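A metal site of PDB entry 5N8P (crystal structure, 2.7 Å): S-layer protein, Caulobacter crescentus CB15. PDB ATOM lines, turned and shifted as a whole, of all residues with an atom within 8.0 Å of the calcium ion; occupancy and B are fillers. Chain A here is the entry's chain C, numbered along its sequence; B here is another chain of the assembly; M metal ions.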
ATOM      1  N   SER A 253     -27.554   5.361  -0.892  1.00  0.00           N
ATOM      2  CA  SER A 253     -26.799   4.979   0.285  1.00  0.00           C
ATOM      3  C   SER A 253     -25.332   5.353   0.306  1.00  0.00           C
ATOM      4  O   SER A 253     -24.606   4.908  -0.561  1.00  0.00           O
ATOM      5  CB  SER A 253     -26.885   3.469   0.489  1.00  0.00           C
ATOM      6  OG  SER A 253     -28.028   3.144   1.210  1.00  0.00           O
ATOM      7  N   LEU A 254     -24.895   6.097   1.302  1.00  0.00           N
ATOM      8  CA  LEU A 254     -23.477   6.406   1.519  1.00  0.00           C
ATOM      9  C   LEU A 254     -22.721   5.197   2.036  1.00  0.00           C
ATOM     10  O   LEU A 254     -23.303   4.400   2.739  1.00  0.00           O
ATOM     11  CB  LEU A 254     -23.277   7.587   2.466  1.00  0.00           C
ATOM     12  CG  LEU A 254     -23.337   9.009   1.878  1.00  0.00           C
ATOM     13  CD1 LEU A 254     -24.741   9.430   1.566  1.00  0.00           C
ATOM     14  CD2 LEU A 254     -22.719  10.018   2.832  1.00  0.00           C
ATOM     15  N   THR A 255     -21.442   5.072   1.678  1.00  0.00           N
ATOM     16  CA  THR A 255     -20.554   3.949   2.123  1.00  0.00           C
ATOM     17  C   THR A 255     -19.390   4.474   2.961  1.00  0.00           C
ATOM     18  O   THR A 255     -19.214   5.693   3.057  1.00  0.00           O
ATOM     19  CB  THR A 255     -19.935   3.198   0.956  1.00  0.00           C
ATOM     20  OG1 THR A 255     -18.849   3.979   0.431  1.00  0.00           O
ATOM     21  CG2 THR A 255     -20.991   2.923  -0.118  1.00  0.00           C
ATOM     22  N   THR A 256     -18.556   3.594   3.511  1.00  0.00           N
ATOM     23  CA  THR A 256     -17.413   4.091   4.260  1.00  0.00           C
ATOM     24  C   THR A 256     -16.335   4.721   3.329  1.00  0.00           C
ATOM     25  O   THR A 256     -15.290   5.148   3.830  1.00  0.00           O
ATOM     26  CB  THR A 256     -16.733   2.989   5.104  1.00  0.00           C
ATOM     27  OG1 THR A 256     -16.243   1.957   4.231  1.00  0.00           O
ATOM     28  CG2 THR A 256     -17.655   2.462   6.103  1.00  0.00           C
ATOM     29  N   GLY A 257     -16.627   4.800   2.030  1.00  0.00           N
ATOM     30  CA  GLY A 257     -15.706   5.433   1.065  1.00  0.00           C
ATOM     31  C   GLY A 257     -15.930   6.914   0.715  1.00  0.00           C
ATOM     32  O   GLY A 257     -16.417   7.713   1.526  1.00  0.00           O
ATOM     33  N   THR A 258     -15.532   7.285  -0.500  1.00  0.00           N
ATOM     34  CA  THR A 258     -15.866   8.595  -1.025  1.00  0.00           C
ATOM     35  C   THR A 258     -16.997   8.450  -2.036  1.00  0.00           C
ATOM     36  O   THR A 258     -16.827   7.836  -3.082  1.00  0.00           O
ATOM     37  CB  THR A 258     -14.630   9.274  -1.633  1.00  0.00           C
ATOM     38  OG1 THR A 258     -13.712   9.529  -0.574  1.00  0.00           O
ATOM     39  CG2 THR A 258     -14.980  10.560  -2.301  1.00  0.00           C
ATOM     40  N   ASP A 259     -18.139   9.033  -1.718  1.00  0.00           N
ATOM     41  CA  ASP A 259     -19.336   8.842  -2.515  1.00  0.00           C
ATOM     42  C   ASP A 259     -19.632  10.049  -3.368  1.00  0.00           C
ATOM     43  O   ASP A 259     -19.412  11.195  -2.950  1.00  0.00           O
ATOM     44  CB  ASP A 259     -20.517   8.542  -1.604  1.00  0.00           C
ATOM     45  CG  ASP A 259     -20.212   7.382  -0.660  1.00  0.00           C
ATOM     46  OD1 ASP A 259     -20.200   6.206  -1.098  1.00  0.00           O
ATOM     47  OD2 ASP A 259     -19.959   7.645   0.536  1.00  0.00           O
ATOM     48  N   THR A 260     -20.082   9.763  -4.588  1.00  0.00           N
ATOM     49  CA  THR A 260     -20.504  10.826  -5.491  1.00  0.00           C
ATOM     50  C   THR A 260     -21.945  10.560  -5.937  1.00  0.00           C
ATOM     51  O   THR A 260     -22.214   9.858  -6.919  1.00  0.00           O
ATOM     52  CB  THR A 260     -19.515  10.989  -6.668  1.00  0.00           C
ATOM     53  OG1 THR A 260     -18.168  11.003  -6.154  1.00  0.00           O
ATOM     54  CG2 THR A 260     -19.807  12.323  -7.423  1.00  0.00           C
ATOM     55  N   LEU A 261     -22.898  11.122  -5.175  1.00  0.00           N
ATOM     56  CA  LEU A 261     -24.293  10.773  -5.335  1.00  0.00           C
ATOM     57  C   LEU A 261     -25.106  11.951  -5.844  1.00  0.00           C
ATOM     58  O   LEU A 261     -24.928  13.094  -5.398  1.00  0.00           O
ATOM     59  CB  LEU A 261     -24.856  10.266  -4.013  1.00  0.00           C
ATOM     60  CG  LEU A 261     -24.144   9.040  -3.365  1.00  0.00           C
ATOM     61  CD1 LEU A 261     -24.791   8.654  -2.070  1.00  0.00           C
ATOM     62  CD2 LEU A 261     -24.037   7.839  -4.298  1.00  0.00           C
ATOM     63  N   VAL A 271     -29.142   8.272   2.467  1.00  0.00           N
ATOM     64  CA  VAL A 271     -28.908   7.613   3.763  1.00  0.00           C
ATOM     65  C   VAL A 271     -27.446   7.564   4.170  1.00  0.00           C
ATOM     66  O   VAL A 271     -26.640   7.009   3.477  1.00  0.00           O
ATOM     67  CB  VAL A 271     -29.567   6.212   3.834  1.00  0.00           C
ATOM     68  CG1 VAL A 271     -29.332   5.568   5.224  1.00  0.00           C
ATOM     69  CG2 VAL A 271     -31.067   6.283   3.568  1.00  0.00           C
ATOM     70  N   ALA A 272     -27.143   8.168   5.290  1.00  0.00           N
ATOM     71  CA  ALA A 272     -25.778   8.202   5.787  1.00  0.00           C
ATOM     72  C   ALA A 272     -25.622   7.522   7.116  1.00  0.00           C
ATOM     73  O   ALA A 272     -25.190   8.161   8.094  1.00  0.00           O
ATOM     74  CB  ALA A 272     -25.261   9.656   5.807  1.00  0.00           C
ATOM     75  N   ALA A 279     -18.654   5.314  10.377  1.00  0.00           N
ATOM     76  CA  ALA A 279     -19.491   6.367   9.783  1.00  0.00           C
ATOM     77  C   ALA A 279     -19.504   6.283   8.261  1.00  0.00           C
ATOM     78  O   ALA A 279     -18.485   5.878   7.657  1.00  0.00           O
ATOM     79  CB  ALA A 279     -18.951   7.713  10.220  1.00  0.00           C
ATOM     80  N   THR A 280     -20.620   6.652   7.629  1.00  0.00           N
ATOM     81  CA  THR A 280     -20.615   6.708   6.131  1.00  0.00           C
ATOM     82  C   THR A 280     -20.578   8.105   5.511  1.00  0.00           C
ATOM     83  O   THR A 280     -20.398   8.235   4.307  1.00  0.00           O
ATOM     84  CB  THR A 280     -21.685   5.839   5.458  1.00  0.00           C
ATOM     85  OG1 THR A 280     -22.966   6.402   5.651  1.00  0.00           O
ATOM     86  CG2 THR A 280     -21.620   4.420   5.968  1.00  0.00           C
ATOM     87  N   LEU A 281     -20.734   9.149   6.323  1.00  0.00           N
ATOM     88  CA  LEU A 281     -20.381  10.475   5.872  1.00  0.00           C
ATOM     89  C   LEU A 281     -18.894  10.672   6.209  1.00  0.00           C
ATOM     90  O   LEU A 281     -18.497  10.709   7.383  1.00  0.00           O
ATOM     91  CB  LEU A 281     -21.284  11.524   6.532  1.00  0.00           C
ATOM     92  CG  LEU A 281     -21.279  12.871   5.776  1.00  0.00           C
ATOM     93  CD1 LEU A 281     -22.224  12.920   4.556  1.00  0.00           C
ATOM     94  CD2 LEU A 281     -21.713  13.917   6.805  1.00  0.00           C
ATOM     95  N   THR A 282     -18.092  10.730   5.158  1.00  0.00           N
ATOM     96  CA  THR A 282     -16.634  10.620   5.253  1.00  0.00           C
ATOM     97  C   THR A 282     -15.976  11.556   4.244  1.00  0.00           C
ATOM     98  O   THR A 282     -16.635  12.115   3.373  1.00  0.00           O
ATOM     99  CB  THR A 282     -16.138   9.230   4.888  1.00  0.00           C
ATOM    100  OG1 THR A 282     -16.922   8.766   3.786  1.00  0.00           O
ATOM    101  CG2 THR A 282     -16.315   8.275   6.030  1.00  0.00           C
ATOM    102  N   VAL A 283     -14.651  11.673   4.353  1.00  0.00           N
ATOM    103  CA  VAL A 283     -13.888  12.612   3.567  1.00  0.00           C
ATOM    104  C   VAL A 283     -14.191  12.570   2.064  1.00  0.00           C
ATOM    105  O   VAL A 283     -14.263  11.477   1.487  1.00  0.00           O
ATOM    106  CB  VAL A 283     -12.373  12.652   3.953  1.00  0.00           C
ATOM    107  CG1 VAL A 283     -12.142  12.225   5.397  1.00  0.00           C
ATOM    108  CG2 VAL A 283     -11.538  11.882   2.968  1.00  0.00           C
ATOM    109  N   GLY A 284     -14.452  13.733   1.469  1.00  0.00           N
ATOM    110  CA  GLY A 284     -14.662  13.864   0.042  1.00  0.00           C
ATOM    111  C   GLY A 284     -16.056  13.561  -0.499  1.00  0.00           C
ATOM    112  O   GLY A 284     -16.339  13.852  -1.677  1.00  0.00           O
ATOM    113  N   ASP A 285     -16.918  12.996   0.349  1.00  0.00           N
ATOM    114  CA  ASP A 285     -18.307  12.714  -0.017  1.00  0.00           C
ATOM    115  C   ASP A 285     -18.968  13.949  -0.652  1.00  0.00           C
ATOM    116  O   ASP A 285     -19.000  15.028  -0.052  1.00  0.00           O
ATOM    117  CB  ASP A 285     -19.131  12.317   1.225  1.00  0.00           C
ATOM    118  CG  ASP A 285     -18.911  10.887   1.686  1.00  0.00           C
ATOM    119  OD1 ASP A 285     -19.328  10.563   2.815  1.00  0.00           O
ATOM    120  OD2 ASP A 285     -18.325  10.056   0.941  1.00  0.00           O
ATOM    121  N   THR A 286     -19.465  13.804  -1.879  1.00  0.00           N
ATOM    122  CA  THR A 286     -20.215  14.931  -2.428  1.00  0.00           C
ATOM    123  C   THR A 286     -21.620  14.500  -2.853  1.00  0.00           C
ATOM    124  O   THR A 286     -21.792  13.525  -3.629  1.00  0.00           O
ATOM    125  CB  THR A 286     -19.458  15.756  -3.533  1.00  0.00           C
ATOM    126  OG1 THR A 286     -19.443  15.016  -4.751  1.00  0.00           O
ATOM    127  CG2 THR A 286     -17.995  16.174  -3.106  1.00  0.00           C
ATOM    128  N   LEU A 287     -22.617  15.217  -2.311  1.00  0.00           N
ATOM    129  CA  LEU A 287     -24.028  14.903  -2.532  1.00  0.00           C
ATOM    130  C   LEU A 287     -24.745  16.043  -3.227  1.00  0.00           C
ATOM    131  O   LEU A 287     -24.502  17.237  -2.948  1.00  0.00           O
ATOM    132  CB  LEU A 287     -24.724  14.542  -1.211  1.00  0.00           C
ATOM    133  CG  LEU A 287     -24.010  13.568  -0.265  1.00  0.00           C
ATOM    134  CD1 LEU A 287     -24.739  13.501   1.071  1.00  0.00           C
ATOM    135  CD2 LEU A 287     -23.916  12.178  -0.821  1.00  0.00           C
ATOM    136  N   VAL A 311     -16.243  17.350   2.104  1.00  0.00           N
ATOM    137  CA  VAL A 311     -17.675  17.085   2.018  1.00  0.00           C
ATOM    138  C   VAL A 311     -18.366  18.336   1.520  1.00  0.00           C
ATOM    139  O   VAL A 311     -18.073  19.457   1.995  1.00  0.00           O
ATOM    140  CB  VAL A 311     -18.258  16.582   3.376  1.00  0.00           C
ATOM    141  CG1 VAL A 311     -19.781  16.625   3.414  1.00  0.00           C
ATOM    142  CG2 VAL A 311     -17.753  15.188   3.691  1.00  0.00           C
ATOM    143  N   GLU B 274     -11.119   8.274  -0.091  1.00  0.00           N
ATOM    144  CA  GLU B 274     -10.637   7.412   0.977  1.00  0.00           C
ATOM    145  C   GLU B 274     -11.443   6.140   1.072  1.00  0.00           C
ATOM    146  O   GLU B 274     -12.578   6.102   0.598  1.00  0.00           O
ATOM    147  CB  GLU B 274     -10.728   8.143   2.271  1.00  0.00           C
ATOM    148  CG  GLU B 274      -9.509   9.007   2.505  1.00  0.00           C
ATOM    149  CD  GLU B 274      -9.477   9.624   3.871  1.00  0.00           C
ATOM    150  OE1 GLU B 274     -10.458   9.485   4.657  1.00  0.00           O
ATOM    151  OE2 GLU B 274      -8.443  10.236   4.123  1.00  0.00           O
ATOM    152  N   VAL B 275     -10.842   5.089   1.636  1.00  0.00           N
ATOM    153  CA  VAL B 275     -11.605   3.873   1.909  1.00  0.00           C
ATOM    154  C   VAL B 275     -11.898   3.612   3.380  1.00  0.00           C
ATOM    155  O   VAL B 275     -13.057   3.575   3.765  1.00  0.00           O
ATOM    156  CB  VAL B 275     -11.219   2.663   1.028  1.00  0.00           C
ATOM    157  CG1 VAL B 275     -11.172   1.363   1.824  1.00  0.00           C
ATOM    158  CG2 VAL B 275     -12.235   2.542  -0.112  1.00  0.00           C
HETATM  159 CA    CA M   1     -18.841   8.002   2.244  1.00  0.00          CA
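The calcium ion is bound by the side-chain carboxylate (OD2) of Asp 259, the backbone carbonyl oxygen (O) of Thr 255, the side-chain carboxylate (OD2) of Asp 285, the backbone carbonyl oxygen (O) of Gly 257, the side-chain hydroxyl (OG1) of Thr 282, the backbone carbonyl oxygen (O) of Thr 280 and the side-chain carboxylate (OD1) of Asp 285.
O of Asp 259 is in hydrogen-bond range of N of Thr 286 (2.8 Å).
The backbone NH (N) of Gly 257 is in hydrogen-bond range of the side-chain hydroxyl (OG1) of Thr 255 (2.9 Å).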
